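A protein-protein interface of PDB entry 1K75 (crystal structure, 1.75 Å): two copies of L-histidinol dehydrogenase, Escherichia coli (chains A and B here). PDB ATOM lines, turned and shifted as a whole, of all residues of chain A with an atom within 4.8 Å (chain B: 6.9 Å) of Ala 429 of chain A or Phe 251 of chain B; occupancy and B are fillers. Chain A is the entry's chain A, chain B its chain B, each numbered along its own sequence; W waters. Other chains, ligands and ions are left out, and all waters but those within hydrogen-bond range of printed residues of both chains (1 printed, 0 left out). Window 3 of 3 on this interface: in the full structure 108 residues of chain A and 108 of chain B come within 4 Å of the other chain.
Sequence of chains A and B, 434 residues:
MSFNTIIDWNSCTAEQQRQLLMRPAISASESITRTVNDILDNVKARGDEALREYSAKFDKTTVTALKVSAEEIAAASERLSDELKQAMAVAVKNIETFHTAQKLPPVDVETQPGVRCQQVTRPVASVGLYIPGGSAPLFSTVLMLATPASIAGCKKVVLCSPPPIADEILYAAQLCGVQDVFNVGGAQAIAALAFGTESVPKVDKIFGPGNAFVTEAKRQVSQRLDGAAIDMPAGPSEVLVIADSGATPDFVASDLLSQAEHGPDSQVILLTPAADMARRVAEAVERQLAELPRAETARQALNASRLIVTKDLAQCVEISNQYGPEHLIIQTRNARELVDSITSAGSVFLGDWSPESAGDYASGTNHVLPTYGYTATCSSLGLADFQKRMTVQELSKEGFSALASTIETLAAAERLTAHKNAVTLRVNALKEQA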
ATOM      1  N   LEU A 425     -26.034 -20.311  -8.242  1.00  0.00           N
ATOM      2  CA  LEU A 425     -26.237 -20.428  -6.792  1.00  0.00           C
ATOM      3  C   LEU A 425     -25.768 -21.797  -6.298  1.00  0.00           C
ATOM      4  O   LEU A 425     -25.139 -21.897  -5.242  1.00  0.00           O
ATOM      5  CB  LEU A 425     -27.714 -20.246  -6.447  1.00  0.00           C
ATOM      6  CG  LEU A 425     -28.183 -18.793  -6.542  1.00  0.00           C
ATOM      7  CD1 LEU A 425     -29.737 -18.745  -6.574  1.00  0.00           C
ATOM      8  CD2 LEU A 425     -27.657 -18.021  -5.305  1.00  0.00           C
ATOM      9  N   ARG A 426     -26.079 -22.849  -7.057  1.00  0.00           N
ATOM     10  CA  ARG A 426     -25.699 -24.191  -6.638  1.00  0.00           C
ATOM     11  C   ARG A 426     -24.212 -24.428  -6.781  1.00  0.00           C
ATOM     12  O   ARG A 426     -23.593 -25.057  -5.905  1.00  0.00           O
ATOM     13  CB  ARG A 426     -26.508 -25.247  -7.423  1.00  0.00           C
ATOM     14  CG  ARG A 426     -28.010 -25.266  -7.021  1.00  0.00           C
ATOM     15  CD  ARG A 426     -28.874 -26.031  -8.041  1.00  0.00           C
ATOM     16  NE  ARG A 426     -30.234 -26.280  -7.556  1.00  0.00           N
ATOM     17  CZ  ARG A 426     -31.246 -25.406  -7.584  1.00  0.00           C
ATOM     18  NH1 ARG A 426     -31.090 -24.173  -8.072  1.00  0.00           N
ATOM     19  NH2 ARG A 426     -32.442 -25.796  -7.165  1.00  0.00           N
ATOM     20  N   VAL A 427     -23.644 -23.979  -7.898  1.00  0.00           N
ATOM     21  CA  VAL A 427     -22.201 -24.134  -8.112  1.00  0.00           C
ATOM     22  C   VAL A 427     -21.447 -23.447  -6.945  1.00  0.00           C
ATOM     23  O   VAL A 427     -20.476 -23.995  -6.417  1.00  0.00           O
ATOM     24  CB  VAL A 427     -21.782 -23.491  -9.461  1.00  0.00           C
ATOM     25  CG1 VAL A 427     -20.249 -23.384  -9.545  1.00  0.00           C
ATOM     26  CG2 VAL A 427     -22.305 -24.364 -10.630  1.00  0.00           C
ATOM     27  N   ASN A 428     -21.899 -22.255  -6.543  1.00  0.00           N
ATOM     28  CA  ASN A 428     -21.217 -21.537  -5.458  1.00  0.00           C
ATOM     29  C   ASN A 428     -21.367 -22.219  -4.100  1.00  0.00           C
ATOM     30  O   ASN A 428     -20.424 -22.210  -3.295  1.00  0.00           O
ATOM     31  CB  ASN A 428     -21.703 -20.097  -5.364  1.00  0.00           C
ATOM     32  CG  ASN A 428     -21.133 -19.235  -6.476  1.00  0.00           C
ATOM     33  OD1 ASN A 428     -20.094 -19.580  -7.076  1.00  0.00           O
ATOM     34  ND2 ASN A 428     -21.801 -18.132  -6.776  1.00  0.00           N
ATOM     35  N   ALA A 429     -22.533 -22.810  -3.847  1.00  0.00           N
ATOM     36  CA  ALA A 429     -22.750 -23.518  -2.580  1.00  0.00           C
ATOM     37  C   ALA A 429     -21.825 -24.744  -2.532  1.00  0.00           C
ATOM     38  O   ALA A 429     -21.210 -25.028  -1.500  1.00  0.00           O
ATOM     39  CB  ALA A 429     -24.222 -23.949  -2.456  1.00  0.00           C
ATOM     40  N   LEU A 430     -21.706 -25.443  -3.652  1.00  0.00           N
ATOM     41  CA  LEU A 430     -20.839 -26.624  -3.717  1.00  0.00           C
ATOM     42  C   LEU A 430     -19.369 -26.226  -3.530  1.00  0.00           C
ATOM     43  O   LEU A 430     -18.602 -26.970  -2.879  1.00  0.00           O
ATOM     44  CB  LEU A 430     -21.052 -27.376  -5.033  1.00  0.00           C
ATOM     45  CG  LEU A 430     -22.383 -28.161  -5.103  1.00  0.00           C
ATOM     46  CD1 LEU A 430     -22.545 -28.690  -6.529  1.00  0.00           C
ATOM     47  CD2 LEU A 430     -22.428 -29.323  -4.098  1.00  0.00           C
ATOM     48  N   LYS A 431     -18.972 -25.072  -4.077  1.00  0.00           N
ATOM     49  CA  LYS A 431     -17.581 -24.602  -3.899  1.00  0.00           C
ATOM     50  C   LYS A 431     -17.314 -24.318  -2.410  1.00  0.00           C
ATOM     51  O   LYS A 431     -16.217 -24.606  -1.891  1.00  0.00           O
ATOM     52  CB  LYS A 431     -17.315 -23.319  -4.691  1.00  0.00           C
ATOM     53  CG  LYS A 431     -17.074 -23.555  -6.150  1.00  0.00           C
ATOM     54  CD  LYS A 431     -16.919 -22.220  -6.879  1.00  0.00           C
ATOM     55  CE  LYS A 431     -16.768 -22.403  -8.384  1.00  0.00           C
ATOM     56  NZ  LYS A 431     -16.477 -21.111  -9.055  1.00  0.00           N
ATOM     57  N   GLU A 432     -18.295 -23.731  -1.733  1.00  0.00           N
ATOM     58  CA  GLU A 432     -18.144 -23.420  -0.299  1.00  0.00           C
ATOM     59  C   GLU A 432     -18.021 -24.675   0.565  1.00  0.00           C
ATOM     60  O   GLU A 432     -17.317 -24.675   1.582  1.00  0.00           O
ATOM     61  CB  GLU A 432     -19.335 -22.602   0.207  1.00  0.00           C
ATOM     62  CG  GLU A 432     -19.261 -21.149  -0.139  1.00  0.00           C
ATOM     63  CD  GLU A 432     -18.019 -20.497   0.463  1.00  0.00           C
ATOM     64  OE1 GLU A 432     -17.903 -20.487   1.712  1.00  0.00           O
ATOM     65  OE2 GLU A 432     -17.164 -20.002  -0.318  1.00  0.00           O
ATOM     66  N   GLN A 433     -18.683 -25.745   0.149  1.00  0.00           N
ATOM     67  CA  GLN A 433     -18.691 -26.992   0.909  1.00  0.00           C
ATOM     68  C   GLN A 433     -17.607 -27.965   0.508  1.00  0.00           C
ATOM     69  O   GLN A 433     -17.468 -29.011   1.131  1.00  0.00           O
ATOM     70  CB  GLN A 433     -20.044 -27.700   0.737  1.00  0.00           C
ATOM     71  CG  GLN A 433     -21.227 -26.946   1.287  1.00  0.00           C
ATOM     72  CD  GLN A 433     -22.547 -27.587   0.891  1.00  0.00           C
ATOM     73  OE1 GLN A 433     -22.591 -28.748   0.459  1.00  0.00           O
ATOM     74  NE2 GLN A 433     -23.634 -26.834   1.034  1.00  0.00           N
ATOM     75  N   VAL B 241     -43.083 -26.442  -6.095  1.00  0.00           N
ATOM     76  CA  VAL B 241     -41.929 -26.946  -5.357  1.00  0.00           C
ATOM     77  C   VAL B 241     -42.444 -27.412  -3.999  1.00  0.00           C
ATOM     78  O   VAL B 241     -43.223 -26.701  -3.377  1.00  0.00           O
ATOM     79  CB  VAL B 241     -40.896 -25.822  -5.105  1.00  0.00           C
ATOM     80  CG1 VAL B 241     -39.679 -26.390  -4.279  1.00  0.00           C
ATOM     81  CG2 VAL B 241     -40.465 -25.192  -6.439  1.00  0.00           C
ATOM     82  N   ALA B 247     -34.346 -27.806   3.236  1.00  0.00           N
ATOM     83  CA  ALA B 247     -34.145 -27.102   1.956  1.00  0.00           C
ATOM     84  C   ALA B 247     -33.358 -25.799   2.108  1.00  0.00           C
ATOM     85  O   ALA B 247     -33.291 -25.220   3.183  1.00  0.00           O
ATOM     86  CB  ALA B 247     -35.556 -26.787   1.304  1.00  0.00           C
ATOM     87  N   THR B 248     -32.775 -25.323   1.014  1.00  0.00           N
ATOM     88  CA  THR B 248     -32.007 -24.078   1.021  1.00  0.00           C
ATOM     89  C   THR B 248     -32.908 -23.015   0.360  1.00  0.00           C
ATOM     90  O   THR B 248     -33.235 -23.130  -0.835  1.00  0.00           O
ATOM     91  CB  THR B 248     -30.702 -24.267   0.209  1.00  0.00           C
ATOM     92  OG1 THR B 248     -29.859 -25.187   0.911  1.00  0.00           O
ATOM     93  CG2 THR B 248     -29.948 -22.961   0.038  1.00  0.00           C
ATOM     94  N   PRO B 249     -33.345 -21.999   1.133  1.00  0.00           N
ATOM     95  CA  PRO B 249     -34.219 -20.947   0.609  1.00  0.00           C
ATOM     96  C   PRO B 249     -33.810 -20.403  -0.748  1.00  0.00           C
ATOM     97  O   PRO B 249     -34.666 -20.265  -1.626  1.00  0.00           O
ATOM     98  CB  PRO B 249     -34.199 -19.890   1.720  1.00  0.00           C
ATOM     99  CG  PRO B 249     -34.097 -20.747   2.973  1.00  0.00           C
ATOM    100  CD  PRO B 249     -33.006 -21.730   2.546  1.00  0.00           C
ATOM    101  N   ASP B 250     -32.520 -20.101  -0.948  1.00  0.00           N
ATOM    102  CA  ASP B 250     -32.106 -19.579  -2.243  1.00  0.00           C
ATOM    103  C   ASP B 250     -32.313 -20.549  -3.378  1.00  0.00           C
ATOM    104  O   ASP B 250     -32.583 -20.111  -4.493  1.00  0.00           O
ATOM    105  CB  ASP B 250     -30.631 -19.145  -2.262  1.00  0.00           C
ATOM    106  CG  ASP B 250     -30.434 -17.753  -1.715  1.00  0.00           C
ATOM    107  OD1 ASP B 250     -31.373 -16.934  -1.783  1.00  0.00           O
ATOM    108  OD2 ASP B 250     -29.324 -17.465  -1.237  1.00  0.00           O
ATOM    109  N   PHE B 251     -32.161 -21.851  -3.129  1.00  0.00           N
ATOM    110  CA  PHE B 251     -32.372 -22.833  -4.211  1.00  0.00           C
ATOM    111  C   PHE B 251     -33.869 -22.876  -4.565  1.00  0.00           C
ATOM    112  O   PHE B 251     -34.236 -22.851  -5.743  1.00  0.00           O
ATOM    113  CB  PHE B 251     -31.935 -24.238  -3.783  1.00  0.00           C
ATOM    114  CG  PHE B 251     -30.455 -24.383  -3.546  1.00  0.00           C
ATOM    115  CD1 PHE B 251     -29.574 -23.321  -3.766  1.00  0.00           C
ATOM    116  CD2 PHE B 251     -29.938 -25.607  -3.124  1.00  0.00           C
ATOM    117  CE1 PHE B 251     -28.179 -23.484  -3.563  1.00  0.00           C
ATOM    118  CE2 PHE B 251     -28.548 -25.775  -2.925  1.00  0.00           C
ATOM    119  CZ  PHE B 251     -27.680 -24.720  -3.141  1.00  0.00           C
ATOM    120  N   VAL B 252     -34.726 -22.945  -3.548  1.00  0.00           N
ATOM    121  CA  VAL B 252     -36.179 -22.958  -3.799  1.00  0.00           C
ATOM    122  C   VAL B 252     -36.547 -21.713  -4.596  1.00  0.00           C
ATOM    123  O   VAL B 252     -37.199 -21.791  -5.646  1.00  0.00           O
ATOM    124  CB  VAL B 252     -36.959 -22.955  -2.460  1.00  0.00           C
ATOM    125  CG1 VAL B 252     -38.481 -22.826  -2.718  1.00  0.00           C
ATOM    126  CG2 VAL B 252     -36.629 -24.233  -1.686  1.00  0.00           C
ATOM    127  N   ALA B 253     -36.108 -20.561  -4.110  1.00  0.00           N
ATOM    128  CA  ALA B 253     -36.437 -19.300  -4.774  1.00  0.00           C
ATOM    129  C   ALA B 253     -35.938 -19.273  -6.225  1.00  0.00           C
ATOM    130  O   ALA B 253     -36.642 -18.798  -7.118  1.00  0.00           O
ATOM    131  CB  ALA B 253     -35.834 -18.135  -3.990  1.00  0.00           C
ATOM    132  N   SER B 254     -34.742 -19.813  -6.458  1.00  0.00           N
ATOM    133  CA  SER B 254     -34.201 -19.813  -7.807  1.00  0.00           C
ATOM    134  C   SER B 254     -35.081 -20.587  -8.806  1.00  0.00           C
ATOM    135  O   SER B 254     -35.220 -20.170  -9.967  1.00  0.00           O
ATOM    136  CB  SER B 254     -32.765 -20.363  -7.801  1.00  0.00           C
ATOM    137  OG  SER B 254     -32.732 -21.762  -7.674  1.00  0.00           O
ATOM    138  N   ASP B 255     -35.682 -21.684  -8.360  1.00  0.00           N
ATOM    139  CA  ASP B 255     -36.554 -22.474  -9.223  1.00  0.00           C
ATOM    140  C   ASP B 255     -37.910 -21.783  -9.416  1.00  0.00           C
ATOM    141  O   ASP B 255     -38.491 -21.846 -10.503  1.00  0.00           O
ATOM    142  CB  ASP B 255     -36.728 -23.876  -8.650  1.00  0.00           C
ATOM    143  CG  ASP B 255     -35.489 -24.758  -8.929  1.00  0.00           C
ATOM    144  OD1 ASP B 255     -35.083 -24.842 -10.137  1.00  0.00           O
ATOM    145  OD2 ASP B 255     -34.949 -25.345  -7.957  1.00  0.00           O
ATOM    146  N   LEU B 256     -38.407 -21.130  -8.373  1.00  0.00           N
ATOM    147  CA  LEU B 256     -39.672 -20.391  -8.521  1.00  0.00           C
ATOM    148  C   LEU B 256     -39.438 -19.273  -9.534  1.00  0.00           C
ATOM    149  O   LEU B 256     -40.279 -19.029 -10.421  1.00  0.00           O
ATOM    150  CB  LEU B 256     -40.125 -19.776  -7.190  1.00  0.00           C
ATOM    151  CG  LEU B 256     -40.491 -20.761  -6.057  1.00  0.00           C
ATOM    152  CD1 LEU B 256     -40.942 -19.937  -4.828  1.00  0.00           C
ATOM    153  CD2 LEU B 256     -41.611 -21.714  -6.485  1.00  0.00           C
ATOM    154  N   ALA B 284     -36.016 -14.585  -0.083  1.00  0.00           N
ATOM    155  CA  ALA B 284     -35.040 -14.915  -1.108  1.00  0.00           C
ATOM    156  C   ALA B 284     -35.583 -14.593  -2.504  1.00  0.00           C
ATOM    157  O   ALA B 284     -34.829 -14.169  -3.381  1.00  0.00           O
ATOM    158  CB  ALA B 284     -34.672 -16.399  -1.034  1.00  0.00           C
ATOM    159  N   GLN B 288     -33.625 -12.058  -4.993  1.00  0.00           N
ATOM    160  CA  GLN B 288     -33.119 -12.535  -6.262  1.00  0.00           C
ATOM    161  C   GLN B 288     -33.757 -11.806  -7.413  1.00  0.00           C
ATOM    162  O   GLN B 288     -33.116 -11.542  -8.443  1.00  0.00           O
ATOM    163  CB  GLN B 288     -33.359 -14.026  -6.394  1.00  0.00           C
ATOM    164  CG  GLN B 288     -32.395 -14.836  -5.526  1.00  0.00           C
ATOM    165  CD  GLN B 288     -32.646 -16.330  -5.616  1.00  0.00           C
ATOM    166  OE1 GLN B 288     -33.062 -16.840  -6.637  1.00  0.00           O
ATOM    167  NE2 GLN B 288     -32.359 -17.032  -4.537  1.00  0.00           N
ATOM    168  N   ILE B 329     -40.972 -29.985  -8.323  1.00  0.00           N
ATOM    169  CA  ILE B 329     -39.629 -29.981  -7.782  1.00  0.00           C
ATOM    170  C   ILE B 329     -39.698 -30.387  -6.308  1.00  0.00           C
ATOM    171  O   ILE B 329     -40.367 -29.714  -5.514  1.00  0.00           O
ATOM    172  CB  ILE B 329     -39.007 -28.583  -7.960  1.00  0.00           C
ATOM    173  CG1 ILE B 329     -38.919 -28.292  -9.477  1.00  0.00           C
ATOM    174  CG2 ILE B 329     -37.599 -28.542  -7.316  1.00  0.00           C
ATOM    175  CD1 ILE B 329     -38.204 -26.978  -9.820  1.00  0.00           C
ATOM    176  N   GLN B 331     -37.635 -30.795  -3.041  1.00  0.00           N
ATOM    177  CA  GLN B 331     -36.445 -30.475  -2.274  1.00  0.00           C
ATOM    178  C   GLN B 331     -36.733 -30.881  -0.829  1.00  0.00           C
ATOM    179  O   GLN B 331     -36.979 -30.051   0.042  1.00  0.00           O
ATOM    180  CB  GLN B 331     -36.101 -28.985  -2.442  1.00  0.00           C
ATOM    181  CG  GLN B 331     -35.382 -28.737  -3.802  1.00  0.00           C
ATOM    182  CD  GLN B 331     -35.201 -27.269  -4.157  1.00  0.00           C
ATOM    183  OE1 GLN B 331     -35.045 -26.418  -3.284  1.00  0.00           O
ATOM    184  NE2 GLN B 331     -35.196 -26.969  -5.453  1.00  0.00           N
ATOM    185  N   GLY B 351     -34.298 -33.461  -5.250  1.00  0.00           N
ATOM    186  CA  GLY B 351     -33.137 -33.003  -4.497  1.00  0.00           C
ATOM    187  C   GLY B 351     -32.609 -31.620  -4.813  1.00  0.00           C
ATOM    188  O   GLY B 351     -33.083 -30.918  -5.714  1.00  0.00           O
ATOM    189  N   ASP B 352     -31.578 -31.236  -4.080  1.00  0.00           N
ATOM    190  CA  ASP B 352     -31.025 -29.908  -4.227  1.00  0.00           C
ATOM    191  C   ASP B 352     -30.263 -29.619  -5.511  1.00  0.00           C
ATOM    192  O   ASP B 352     -30.104 -28.461  -5.863  1.00  0.00           O
ATOM    193  CB  ASP B 352     -30.054 -29.594  -3.091  1.00  0.00           C
ATOM    194  CG  ASP B 352     -30.719 -29.462  -1.739  1.00  0.00           C
ATOM    195  OD1 ASP B 352     -31.945 -29.280  -1.654  1.00  0.00           O
ATOM    196  OD2 ASP B 352     -29.979 -29.529  -0.732  1.00  0.00           O
ATOM    197  N   TRP B 353     -29.786 -30.653  -6.207  1.00  0.00           N
ATOM    198  CA  TRP B 353     -28.940 -30.398  -7.359  1.00  0.00           C
ATOM    199  C   TRP B 353     -29.606 -30.667  -8.676  1.00  0.00           C
ATOM    200  O   TRP B 353     -28.918 -30.897  -9.665  1.00  0.00           O
ATOM    201  CB  TRP B 353     -27.637 -31.231  -7.234  1.00  0.00           C
ATOM    202  CG  TRP B 353     -27.113 -31.166  -5.826  1.00  0.00           C
ATOM    203  CD1 TRP B 353     -27.160 -32.160  -4.899  1.00  0.00           C
ATOM    204  CD2 TRP B 353     -26.612 -30.007  -5.153  1.00  0.00           C
ATOM    205  NE1 TRP B 353     -26.728 -31.682  -3.678  1.00  0.00           N
ATOM    206  CE2 TRP B 353     -26.389 -30.366  -3.809  1.00  0.00           C
ATOM    207  CE3 TRP B 353     -26.335 -28.692  -5.557  1.00  0.00           C
ATOM    208  CZ2 TRP B 353     -25.910 -29.462  -2.862  1.00  0.00           C
ATOM    209  CZ3 TRP B 353     -25.857 -27.785  -4.608  1.00  0.00           C
ATOM    210  CH2 TRP B 353     -25.654 -28.180  -3.273  1.00  0.00           C
ATOM    211  N   PRO B 355     -31.946 -28.541 -10.536  1.00  0.00           N
ATOM    212  CA  PRO B 355     -32.725 -27.342 -10.862  1.00  0.00           C
ATOM    213  C   PRO B 355     -33.567 -27.551 -12.112  1.00  0.00           C
ATOM    214  O   PRO B 355     -33.247 -28.373 -12.953  1.00  0.00           O
ATOM    215  CB  PRO B 355     -31.664 -26.292 -11.103  1.00  0.00           C
ATOM    216  CG  PRO B 355     -30.459 -27.129 -11.619  1.00  0.00           C
ATOM    217  CD  PRO B 355     -30.496 -28.289 -10.663  1.00  0.00           C
HETATM  218  O   HOH W   1     -33.425 -28.644  -7.181  1.00  0.00           O
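NH1 of Arg 426 of chain A is in hydrogen-bond range of OG of Ser 254 of chain B, 2.9 Å away. The guanidinium group of Arg 426 of chain A lies within salt-bridge range of the side-chain carboxylate of Asp 255 of chain B (2.7 Å). The guanidinium group (NH2) of Arg 426 of chain A lies close to the side-chain amide nitrogen (NE2) of Gln 331 of chain B (3.4 Å). The guanidinium group of Arg 426 of chain A lies within hydrogen-bond range of the backbone carbonyl oxygen of Asp 352 of chain B.
The side-chain carboxylate (OD1) of Asp 250 of chain B sits at hydrogen-bond distance from the side-chain amide nitrogen (NE2) of Gln 288 of chain B, at 2.9 Å. O of Phe 251 of chain B sits at hydrogen-bond distance from OG of Ser 254 of chain B (2.7 Å). N of Val 252 of chain B lies close to OE1 of Gln 331 of chain B (3.5 Å). OE1 of Gln 288 of chain B sits close to N of Ser 254 of chain B (3.4 Å). The side-chain carboxylate (OD2) of Asp 255 of chain B is in hydrogen-bond range of the side-chain amide nitrogen (NE2) of Gln 331 of chain B (3.0 Å).
Among the printed residues, pairs that only touch across the chains: Leu 430 of chain A with Trp 353 of chain B (3.5 Å), Ala 429 of chain A with Phe 251 of chain B (3.6 Å), Leu 425 of chain A with Ser 254 of chain B (3.6 Å), Arg 426 of chain A with Pro 355 of chain B (3.7 Å), Arg 426 of chain A with Phe 251 of chain B (3.7 Å), Leu 425 of chain A with Gln 288 of chain B (3.7 Å), Arg 426 of chain A with Trp 353 of chain B (3.8 Å), Leu 425 of chain A with Asp 250 of chain B (3.8 Å) and Leu 425 of chain A with Phe 251 of chain B (3.8 Å).
Ala 429 of chain A touches one residue of chain B. Of the printed residues of chain B, Leu 430 of chain A touches Trp 353 (3.5 Å). Gln 433 of chain A touches none of the printed residues of chain B. Printed residues of chain A within 4 Å of Asp 250 of chain B: Leu 425 (3.8 Å). Of chain A, only Leu 425, Arg 426 and Ala 429 come within 4 Å of Phe 251 of chain B. Of the printed residues of chain A, Ser 254 of chain B touches Leu 425 (3.6 Å) and Arg 426 (2.9 Å). Printed residues of chain A within 4 Å of Asp 352 of chain B: Arg 426 (2.8 Å). Printed residues of chain A within 4 Å of Pro 355 of chain B: Arg 426. The nearest residue of chain B that does not touch Ala 429 of chain A is Trp 353 of chain B (4.5 Å). The nearest printed residue of chain A that does not touch Phe 251 of chain B is Leu 430 of chain A (6.0 Å).
Of the 9 printed residues of chain A, 4 touch a printed residue of chain B. Hydrophobic or aromatic side chains of chain A that line the printed part of chain B: Leu 425, Ala 429 and Leu 430. Along chain A the printed residues that touch a printed residue of chain B span positions 425 to 430. Hydrophobic or aromatic side chains of chain B that line the printed part of chain A: Phe 251, Trp 353 and Pro 355.
No position is printed for both chains. Of the 13 pairs that touch across the chains among the printed residues, none has its exchanged pair printed and touching as well.
Water W1 lies within hydrogen-bond range of the backbone carbonyl oxygen (O) of Gly 351 of chain B, the side-chain amide nitrogen (NE2) of Gln 331 of chain B and the guanidinium group (NH2) of Arg 426 of chain A.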
